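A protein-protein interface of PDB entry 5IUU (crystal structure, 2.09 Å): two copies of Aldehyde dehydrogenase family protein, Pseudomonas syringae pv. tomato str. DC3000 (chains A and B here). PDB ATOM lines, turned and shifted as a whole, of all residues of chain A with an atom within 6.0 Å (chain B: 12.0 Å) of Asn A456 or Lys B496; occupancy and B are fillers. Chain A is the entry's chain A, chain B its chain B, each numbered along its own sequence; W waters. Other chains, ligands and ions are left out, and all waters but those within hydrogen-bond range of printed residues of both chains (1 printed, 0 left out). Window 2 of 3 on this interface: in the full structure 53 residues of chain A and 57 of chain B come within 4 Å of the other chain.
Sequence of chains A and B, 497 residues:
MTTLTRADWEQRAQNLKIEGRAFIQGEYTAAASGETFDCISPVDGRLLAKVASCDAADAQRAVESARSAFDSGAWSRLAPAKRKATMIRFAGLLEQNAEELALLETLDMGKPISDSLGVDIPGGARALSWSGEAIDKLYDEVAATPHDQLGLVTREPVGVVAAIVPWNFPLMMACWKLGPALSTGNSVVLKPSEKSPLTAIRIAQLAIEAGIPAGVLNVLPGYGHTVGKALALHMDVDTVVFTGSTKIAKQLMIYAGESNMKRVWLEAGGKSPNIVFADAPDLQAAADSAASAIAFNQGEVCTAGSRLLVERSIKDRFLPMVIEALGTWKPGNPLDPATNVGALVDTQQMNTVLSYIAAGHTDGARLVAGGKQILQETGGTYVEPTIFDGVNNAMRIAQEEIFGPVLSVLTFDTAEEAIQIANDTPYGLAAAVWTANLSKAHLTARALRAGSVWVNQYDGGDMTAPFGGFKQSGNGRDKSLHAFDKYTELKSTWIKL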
ATOM      1  N   ALA A 280     -32.072 -28.306  11.037  1.00  0.00           N
ATOM      2  CA  ALA A 280     -31.886 -26.876  10.801  1.00  0.00           C
ATOM      3  C   ALA A 280     -31.742 -26.154  12.137  1.00  0.00           C
ATOM      4  O   ALA A 280     -32.480 -26.450  13.084  1.00  0.00           O
ATOM      5  CB  ALA A 280     -33.047 -26.282  10.008  1.00  0.00           C
ATOM      6  N   PRO A 281     -30.794 -25.222  12.264  1.00  0.00           N
ATOM      7  CA  PRO A 281     -30.571 -24.602  13.582  1.00  0.00           C
ATOM      8  C   PRO A 281     -31.701 -23.695  14.032  1.00  0.00           C
ATOM      9  O   PRO A 281     -31.907 -23.557  15.243  1.00  0.00           O
ATOM     10  CB  PRO A 281     -29.255 -23.828  13.390  1.00  0.00           C
ATOM     11  CG  PRO A 281     -29.137 -23.617  11.914  1.00  0.00           C
ATOM     12  CD  PRO A 281     -29.797 -24.796  11.261  1.00  0.00           C
ATOM     13  N   ALA A 285     -36.758 -19.547  11.194  1.00  0.00           N
ATOM     14  CA  ALA A 285     -36.160 -18.831  10.068  1.00  0.00           C
ATOM     15  C   ALA A 285     -36.406 -19.566   8.758  1.00  0.00           C
ATOM     16  O   ALA A 285     -36.742 -18.944   7.741  1.00  0.00           O
ATOM     17  CB  ALA A 285     -34.659 -18.633  10.300  1.00  0.00           C
ATOM     18  N   VAL A 433     -30.248 -24.065   1.694  1.00  0.00           N
ATOM     19  CA  VAL A 433     -30.103 -25.277   2.491  1.00  0.00           C
ATOM     20  C   VAL A 433     -30.113 -24.883   3.955  1.00  0.00           C
ATOM     21  O   VAL A 433     -29.456 -23.912   4.344  1.00  0.00           O
ATOM     22  CB  VAL A 433     -28.798 -26.039   2.158  1.00  0.00           C
ATOM     23  CG1 VAL A 433     -28.727 -27.355   2.944  1.00  0.00           C
ATOM     24  CG2 VAL A 433     -28.699 -26.283   0.678  1.00  0.00           C
ATOM     25  N   TRP A 434     -30.829 -25.659   4.771  1.00  0.00           N
ATOM     26  CA  TRP A 434     -30.950 -25.406   6.205  1.00  0.00           C
ATOM     27  C   TRP A 434     -30.540 -26.665   6.958  1.00  0.00           C
ATOM     28  O   TRP A 434     -31.288 -27.647   6.979  1.00  0.00           O
ATOM     29  CB  TRP A 434     -32.378 -24.985   6.569  1.00  0.00           C
ATOM     30  CG  TRP A 434     -32.881 -23.853   5.722  1.00  0.00           C
ATOM     31  CD1 TRP A 434     -33.335 -23.933   4.437  1.00  0.00           C
ATOM     32  CD2 TRP A 434     -32.977 -22.470   6.094  1.00  0.00           C
ATOM     33  NE1 TRP A 434     -33.699 -22.693   3.988  1.00  0.00           N
ATOM     34  CE2 TRP A 434     -33.486 -21.775   4.982  1.00  0.00           C
ATOM     35  CE3 TRP A 434     -32.668 -21.755   7.254  1.00  0.00           C
ATOM     36  CZ2 TRP A 434     -33.708 -20.394   4.997  1.00  0.00           C
ATOM     37  CZ3 TRP A 434     -32.884 -20.377   7.268  1.00  0.00           C
ATOM     38  CH2 TRP A 434     -33.403 -19.713   6.145  1.00  0.00           C
ATOM     39  N   THR A 435     -29.363 -26.633   7.576  1.00  0.00           N
ATOM     40  CA  THR A 435     -28.872 -27.730   8.397  1.00  0.00           C
ATOM     41  C   THR A 435     -27.773 -27.193   9.295  1.00  0.00           C
ATOM     42  O   THR A 435     -26.992 -26.341   8.874  1.00  0.00           O
ATOM     43  CB  THR A 435     -28.337 -28.912   7.561  1.00  0.00           C
ATOM     44  OG1 THR A 435     -27.602 -29.796   8.410  1.00  0.00           O
ATOM     45  CG2 THR A 435     -27.406 -28.449   6.451  1.00  0.00           C
ATOM     46  N   ALA A 436     -27.727 -27.685  10.532  1.00  0.00           N
ATOM     47  CA  ALA A 436     -26.680 -27.329  11.478  1.00  0.00           C
ATOM     48  C   ALA A 436     -25.436 -28.181  11.323  1.00  0.00           C
ATOM     49  O   ALA A 436     -24.455 -27.962  12.046  1.00  0.00           O
ATOM     50  CB  ALA A 436     -27.190 -27.457  12.916  1.00  0.00           C
ATOM     51  N   ALA A 441     -24.007 -29.571   5.302  1.00  0.00           N
ATOM     52  CA  ALA A 441     -24.138 -28.232   4.725  1.00  0.00           C
ATOM     53  C   ALA A 441     -23.212 -28.048   3.526  1.00  0.00           C
ATOM     54  O   ALA A 441     -23.654 -27.650   2.439  1.00  0.00           O
ATOM     55  CB  ALA A 441     -23.843 -27.172   5.779  1.00  0.00           C
ATOM     56  N   TRP A 454     -27.611 -20.462  -0.612  1.00  0.00           N
ATOM     57  CA  TRP A 454     -27.696 -19.847   0.705  1.00  0.00           C
ATOM     58  C   TRP A 454     -27.820 -20.932   1.753  1.00  0.00           C
ATOM     59  O   TRP A 454     -28.634 -21.848   1.603  1.00  0.00           O
ATOM     60  CB  TRP A 454     -28.897 -18.908   0.790  1.00  0.00           C
ATOM     61  CG  TRP A 454     -28.589 -17.695   0.098  1.00  0.00           C
ATOM     62  CD1 TRP A 454     -27.768 -16.710   0.538  1.00  0.00           C
ATOM     63  CD2 TRP A 454     -29.011 -17.321  -1.210  1.00  0.00           C
ATOM     64  NE1 TRP A 454     -27.667 -15.735  -0.407  1.00  0.00           N
ATOM     65  CE2 TRP A 454     -28.426 -16.080  -1.491  1.00  0.00           C
ATOM     66  CE3 TRP A 454     -29.848 -17.895  -2.156  1.00  0.00           C
ATOM     67  CZ2 TRP A 454     -28.643 -15.402  -2.682  1.00  0.00           C
ATOM     68  CZ3 TRP A 454     -30.065 -17.219  -3.337  1.00  0.00           C
ATOM     69  CH2 TRP A 454     -29.464 -15.989  -3.592  1.00  0.00           C
ATOM     70  N   VAL A 455     -27.042 -20.819   2.821  1.00  0.00           N
ATOM     71  CA  VAL A 455     -27.036 -21.828   3.873  1.00  0.00           C
ATOM     72  C   VAL A 455     -27.468 -21.179   5.180  1.00  0.00           C
ATOM     73  O   VAL A 455     -26.834 -20.222   5.653  1.00  0.00           O
ATOM     74  CB  VAL A 455     -25.667 -22.505   4.008  1.00  0.00           C
ATOM     75  CG1 VAL A 455     -25.719 -23.581   5.082  1.00  0.00           C
ATOM     76  CG2 VAL A 455     -25.269 -23.091   2.680  1.00  0.00           C
ATOM     77  N   ASN A 456     -28.560 -21.699   5.751  1.00  0.00           N
ATOM     78  CA  ASN A 456     -29.094 -21.266   7.039  1.00  0.00           C
ATOM     79  C   ASN A 456     -29.535 -19.803   7.011  1.00  0.00           C
ATOM     80  O   ASN A 456     -29.588 -19.136   8.046  1.00  0.00           O
ATOM     81  CB  ASN A 456     -28.083 -21.553   8.154  1.00  0.00           C
ATOM     82  CG  ASN A 456     -27.895 -23.056   8.371  1.00  0.00           C
ATOM     83  OD1 ASN A 456     -28.702 -23.845   7.892  1.00  0.00           O
ATOM     84  ND2 ASN A 456     -26.837 -23.454   9.080  1.00  0.00           N
ATOM     85  N   GLN A 457     -29.879 -19.321   5.819  1.00  0.00           N
ATOM     86  CA  GLN A 457     -30.442 -17.997   5.563  1.00  0.00           C
ATOM     87  C   GLN A 457     -31.014 -18.027   4.149  1.00  0.00           C
ATOM     88  O   GLN A 457     -30.806 -18.988   3.409  1.00  0.00           O
ATOM     89  CB  GLN A 457     -29.391 -16.892   5.710  1.00  0.00           C
ATOM     90  CG  GLN A 457     -28.274 -16.987   4.671  1.00  0.00           C
ATOM     91  CD  GLN A 457     -27.109 -16.047   4.959  1.00  0.00           C
ATOM     92  OE1 GLN A 457     -27.257 -15.051   5.664  1.00  0.00           O
ATOM     93  NE2 GLN A 457     -25.942 -16.368   4.412  1.00  0.00           N
ATOM     94  N   TYR A 458     -31.715 -16.963   3.768  1.00  0.00           N
ATOM     95  CA  TYR A 458     -32.284 -16.864   2.426  1.00  0.00           C
ATOM     96  C   TYR A 458     -32.078 -15.459   1.862  1.00  0.00           C
ATOM     97  O   TYR A 458     -32.144 -14.472   2.598  1.00  0.00           O
ATOM     98  CB  TYR A 458     -33.782 -17.213   2.430  1.00  0.00           C
ATOM     99  CG  TYR A 458     -34.672 -16.287   3.267  1.00  0.00           C
ATOM    100  CD1 TYR A 458     -35.314 -15.193   2.693  1.00  0.00           C
ATOM    101  CD2 TYR A 458     -34.870 -16.519   4.629  1.00  0.00           C
ATOM    102  CE1 TYR A 458     -36.141 -14.362   3.450  1.00  0.00           C
ATOM    103  CE2 TYR A 458     -35.693 -15.698   5.393  1.00  0.00           C
ATOM    104  CZ  TYR A 458     -36.324 -14.617   4.797  1.00  0.00           C
ATOM    105  OH  TYR A 458     -37.140 -13.788   5.547  1.00  0.00           O
ATOM    106  N   ALA B 143     -15.044 -14.355  -0.089  1.00  0.00           N
ATOM    107  CA  ALA B 143     -15.426 -12.942  -0.097  1.00  0.00           C
ATOM    108  C   ALA B 143     -15.228 -12.292   1.269  1.00  0.00           C
ATOM    109  O   ALA B 143     -15.253 -12.954   2.307  1.00  0.00           O
ATOM    110  CB  ALA B 143     -16.889 -12.781  -0.503  1.00  0.00           C
ATOM    111  N   THR B 145     -16.783 -10.542   4.169  1.00  0.00           N
ATOM    112  CA  THR B 145     -18.139 -10.604   4.687  1.00  0.00           C
ATOM    113  C   THR B 145     -18.116 -10.268   6.169  1.00  0.00           C
ATOM    114  O   THR B 145     -17.059 -10.316   6.809  1.00  0.00           O
ATOM    115  CB  THR B 145     -18.750 -12.006   4.488  1.00  0.00           C
ATOM    116  OG1 THR B 145     -17.961 -12.983   5.192  1.00  0.00           O
ATOM    117  CG2 THR B 145     -18.832 -12.373   2.996  1.00  0.00           C
ATOM    118  N   PRO B 146     -19.274  -9.958   6.751  1.00  0.00           N
ATOM    119  CA  PRO B 146     -19.357  -9.833   8.210  1.00  0.00           C
ATOM    120  C   PRO B 146     -18.917 -11.111   8.909  1.00  0.00           C
ATOM    121  O   PRO B 146     -18.873 -12.197   8.315  1.00  0.00           O
ATOM    122  CB  PRO B 146     -20.848  -9.553   8.458  1.00  0.00           C
ATOM    123  CG  PRO B 146     -21.314  -8.890   7.190  1.00  0.00           C
ATOM    124  CD  PRO B 146     -20.539  -9.584   6.090  1.00  0.00           C
ATOM    125  N   HIS B 147     -18.633 -10.978  10.204  1.00  0.00           N
ATOM    126  CA  HIS B 147     -17.973 -12.057  10.934  1.00  0.00           C
ATOM    127  C   HIS B 147     -18.873 -13.275  11.146  1.00  0.00           C
ATOM    128  O   HIS B 147     -18.372 -14.358  11.454  1.00  0.00           O
ATOM    129  CB  HIS B 147     -17.450 -11.539  12.275  1.00  0.00           C
ATOM    130  CG  HIS B 147     -18.459 -11.578  13.388  1.00  0.00           C
ATOM    131  ND1 HIS B 147     -19.605 -10.803  13.395  1.00  0.00           N
ATOM    132  CD2 HIS B 147     -18.484 -12.295  14.539  1.00  0.00           C
ATOM    133  CE1 HIS B 147     -20.294 -11.046  14.498  1.00  0.00           C
ATOM    134  NE2 HIS B 147     -19.635 -11.946  15.210  1.00  0.00           N
ATOM    135  N   ASP B 148     -20.186 -13.129  10.996  1.00  0.00           N
ATOM    136  CA  ASP B 148     -21.106 -14.254  11.109  1.00  0.00           C
ATOM    137  C   ASP B 148     -21.516 -14.804   9.744  1.00  0.00           C
ATOM    138  O   ASP B 148     -22.597 -15.381   9.604  1.00  0.00           O
ATOM    139  CB  ASP B 148     -22.337 -13.836  11.909  1.00  0.00           C
ATOM    140  CG  ASP B 148     -23.146 -12.801  11.194  1.00  0.00           C
ATOM    141  OD1 ASP B 148     -22.578 -12.094  10.338  1.00  0.00           O
ATOM    142  OD2 ASP B 148     -24.355 -12.692  11.472  1.00  0.00           O
ATOM    143  N   GLN B 149     -20.672 -14.628   8.730  1.00  0.00           N
ATOM    144  CA  GLN B 149     -20.945 -15.091   7.379  1.00  0.00           C
ATOM    145  C   GLN B 149     -19.671 -15.687   6.799  1.00  0.00           C
ATOM    146  O   GLN B 149     -18.570 -15.215   7.095  1.00  0.00           O
ATOM    147  CB  GLN B 149     -21.432 -13.944   6.491  1.00  0.00           C
ATOM    148  CG  GLN B 149     -22.755 -13.333   6.881  1.00  0.00           C
ATOM    149  CD  GLN B 149     -23.947 -14.103   6.335  1.00  0.00           C
ATOM    150  OE1 GLN B 149     -23.865 -14.732   5.277  1.00  0.00           O
ATOM    151  NE2 GLN B 149     -25.066 -14.040   7.042  1.00  0.00           N
ATOM    152  N   LEU B 150     -19.819 -16.740   5.995  1.00  0.00           N
ATOM    153  CA  LEU B 150     -18.742 -17.249   5.154  1.00  0.00           C
ATOM    154  C   LEU B 150     -19.225 -17.198   3.713  1.00  0.00           C
ATOM    155  O   LEU B 150     -20.203 -17.868   3.358  1.00  0.00           O
ATOM    156  CB  LEU B 150     -18.338 -18.675   5.549  1.00  0.00           C
ATOM    157  CG  LEU B 150     -17.282 -19.397   4.701  1.00  0.00           C
ATOM    158  CD1 LEU B 150     -15.978 -18.592   4.615  1.00  0.00           C
ATOM    159  CD2 LEU B 150     -17.007 -20.785   5.267  1.00  0.00           C
ATOM    160  N   GLY B 151     -18.561 -16.395   2.893  1.00  0.00           N
ATOM    161  CA  GLY B 151     -18.935 -16.270   1.497  1.00  0.00           C
ATOM    162  C   GLY B 151     -17.902 -16.905   0.590  1.00  0.00           C
ATOM    163  O   GLY B 151     -16.757 -16.453   0.539  1.00  0.00           O
ATOM    164  N   LEU B 152     -18.284 -17.956  -0.124  1.00  0.00           N
ATOM    165  CA  LEU B 152     -17.379 -18.671  -1.010  1.00  0.00           C
ATOM    166  C   LEU B 152     -17.822 -18.457  -2.446  1.00  0.00           C
ATOM    167  O   LEU B 152     -19.015 -18.556  -2.755  1.00  0.00           O
ATOM    168  CB  LEU B 152     -17.349 -20.163  -0.689  1.00  0.00           C
ATOM    169  CG  LEU B 152     -17.036 -20.550   0.751  1.00  0.00           C
ATOM    170  CD1 LEU B 152     -17.207 -22.061   0.943  1.00  0.00           C
ATOM    171  CD2 LEU B 152     -15.617 -20.118   1.117  1.00  0.00           C
ATOM    172  N   SER B 492     -21.773 -18.926  -5.926  1.00  0.00           N
ATOM    173  CA  SER B 492     -21.631 -18.224  -4.655  1.00  0.00           C
ATOM    174  C   SER B 492     -22.378 -18.987  -3.577  1.00  0.00           C
ATOM    175  O   SER B 492     -23.582 -19.226  -3.708  1.00  0.00           O
ATOM    176  CB  SER B 492     -22.189 -16.803  -4.716  1.00  0.00           C
ATOM    177  OG  SER B 492     -21.844 -16.187  -5.919  1.00  0.00           O
ATOM    178  N   THR B 493     -21.678 -19.327  -2.503  1.00  0.00           N
ATOM    179  CA  THR B 493     -22.268 -19.986  -1.346  1.00  0.00           C
ATOM    180  C   THR B 493     -22.149 -19.023  -0.170  1.00  0.00           C
ATOM    181  O   THR B 493     -21.032 -18.686   0.237  1.00  0.00           O
ATOM    182  CB  THR B 493     -21.564 -21.311  -1.066  1.00  0.00           C
ATOM    183  OG1 THR B 493     -21.467 -22.067  -2.281  1.00  0.00           O
ATOM    184  CG2 THR B 493     -22.311 -22.124  -0.015  1.00  0.00           C
ATOM    185  N   TRP B 494     -23.301 -18.569   0.361  1.00  0.00           N
ATOM    186  CA  TRP B 494     -23.372 -17.633   1.485  1.00  0.00           C
ATOM    187  C   TRP B 494     -23.885 -18.373   2.710  1.00  0.00           C
ATOM    188  O   TRP B 494     -25.069 -18.711   2.791  1.00  0.00           O
ATOM    189  CB  TRP B 494     -24.261 -16.430   1.146  1.00  0.00           C
ATOM    190  CG  TRP B 494     -23.737 -15.798  -0.039  1.00  0.00           C
ATOM    191  CD1 TRP B 494     -24.142 -15.990  -1.341  1.00  0.00           C
ATOM    192  CD2 TRP B 494     -22.600 -14.943  -0.090  1.00  0.00           C
ATOM    193  NE1 TRP B 494     -23.337 -15.259  -2.188  1.00  0.00           N
ATOM    194  CE2 TRP B 494     -22.379 -14.618  -1.440  1.00  0.00           C
ATOM    195  CE3 TRP B 494     -21.769 -14.387   0.878  1.00  0.00           C
ATOM    196  CZ2 TRP B 494     -21.331 -13.792  -1.834  1.00  0.00           C
ATOM    197  CZ3 TRP B 494     -20.753 -13.557   0.475  1.00  0.00           C
ATOM    198  CH2 TRP B 494     -20.543 -13.262  -0.866  1.00  0.00           C
ATOM    199  N   ILE B 495     -23.003 -18.573   3.679  1.00  0.00           N
ATOM    200  CA  ILE B 495     -23.256 -19.430   4.826  1.00  0.00           C
ATOM    201  C   ILE B 495     -23.434 -18.556   6.062  1.00  0.00           C
ATOM    202  O   ILE B 495     -22.527 -17.803   6.448  1.00  0.00           O
ATOM    203  CB  ILE B 495     -22.124 -20.452   5.004  1.00  0.00           C
ATOM    204  CG1 ILE B 495     -21.957 -21.253   3.700  1.00  0.00           C
ATOM    205  CG2 ILE B 495     -22.397 -21.342   6.202  1.00  0.00           C
ATOM    206  CD1 ILE B 495     -20.744 -22.193   3.671  1.00  0.00           C
ATOM    207  N   LYS B 496     -24.614 -18.639   6.669  1.00  0.00           N
ATOM    208  CA  LYS B 496     -24.881 -17.954   7.926  1.00  0.00           C
ATOM    209  C   LYS B 496     -24.264 -18.753   9.067  1.00  0.00           C
ATOM    210  O   LYS B 496     -24.528 -19.951   9.205  1.00  0.00           O
ATOM    211  CB  LYS B 496     -26.386 -17.792   8.133  1.00  0.00           C
ATOM    212  CG  LYS B 496     -26.796 -17.205   9.497  1.00  0.00           C
ATOM    213  CD  LYS B 496     -26.407 -15.755   9.621  1.00  0.00           C
ATOM    214  CE  LYS B 496     -27.106 -15.064  10.814  1.00  0.00           C
ATOM    215  NZ  LYS B 496     -28.575 -14.845  10.592  1.00  0.00           N
ATOM    216  N   LEU B 497     -23.413 -18.103   9.854  1.00  0.00           N
ATOM    217  CA  LEU B 497     -22.860 -18.697  11.063  1.00  0.00           C
ATOM    218  C   LEU B 497     -23.525 -18.043  12.282  1.00  0.00           C
ATOM    219  O   LEU B 497     -23.538 -18.618  13.370  1.00  0.00           O
ATOM    220  CB  LEU B 497     -21.341 -18.505  11.107  1.00  0.00           C
ATOM    221  CG  LEU B 497     -20.583 -18.766   9.797  1.00  0.00           C
ATOM    222  CD1 LEU B 497     -19.133 -18.305   9.903  1.00  0.00           C
ATOM    223  CD2 LEU B 497     -20.656 -20.225   9.430  1.00  0.00           C
HETATM  224  O   HOH W   1     -25.284 -21.660  11.032  1.00  0.00           O
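Of the 15 printed residues of chain B, 4 touch a printed residue of chain A. Of the 13 printed residues of chain A, 4 touch a printed residue of chain B. Hydrophobic or aromatic side chains of chain A that line the printed part of chain B: Trp A454 and Val A455. Among the printed residues, no Asp or Glu carboxylate lies within 4 Å of a Lys or Arg side-chain nitrogen of the other chain.
Water W1 bridges the backbone carbonyl oxygen of Lys B496 and the side-chain amide nitrogen of Asn A456.
O of Val A433 lies within hydrogen-bond range of N of Asn A456 (2.8 Å). The side-chain hydroxyl (OG1) of Thr B145 lies within hydrogen-bond range of the backbone carbonyl oxygen (O) of Gln B149. The backbone carbonyl oxygen of Leu B150 lies within hydrogen-bond range of the backbone NH of Ile B495 (2.9 Å). N of Thr A435 is in hydrogen-bond range of OD1 of Asn A456, 2.9 Å away. O of Trp A454 lies within hydrogen-bond range of N of Val A433 (2.7 Å).
No position is printed for both chains. Of the 9 pairs that touch across the chains among the printed residues, none has its exchanged pair printed and touching as well.
Of the printed residues of chain B, Asn A456 touches Lys B496 (3.5 Å). Of the printed residues of chain A, Lys B496 touches Val A455, Asn A456 and Gln A457. No residue of chain B comes within 4 Å of Ala A280. No residue of chain B comes within 4 Å of Ala A285. No residue of chain B comes within 4 Å of Trp A434. Val A455 touches three residues of chain B. Printed residues of chain A within 4 Å of Ile B495: Val A455 (3.8 Å) and Gln A457 (3.7 Å). Printed residues of chain A within 4 Å of Gln B149: Gln A457. Of the printed residues of chain A, Trp B494 touches Trp A454, Val A455 and Gln A457. The nearest printed residue of chain A that does not touch Lys B496 is Trp A454 (6.3 Å).
Among the printed residues, pairs that only touch across the chains: Asn A456 with Lys B496, Trp A454 with Trp B494, Gln A457 with Ile B495 and Val A455 with Ile B495.
The backbone carbonyl oxygen of Val A455 lies within hydrogen-bond range of the backbone NH of Lys B496 (2.9 Å). NE2 of Gln B149 lies within hydrogen-bond range of OE1 of Gln A457 (2.8 Å). N of Val A455 sits at hydrogen-bond distance from O of Trp B494, at 2.9 Å. NE2 of Gln A457 lies close to N of Lys B496 (3.5 Å). O of Trp B494 lies within hydrogen-bond range of NE2 of Gln A457, 3.0 Å away.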
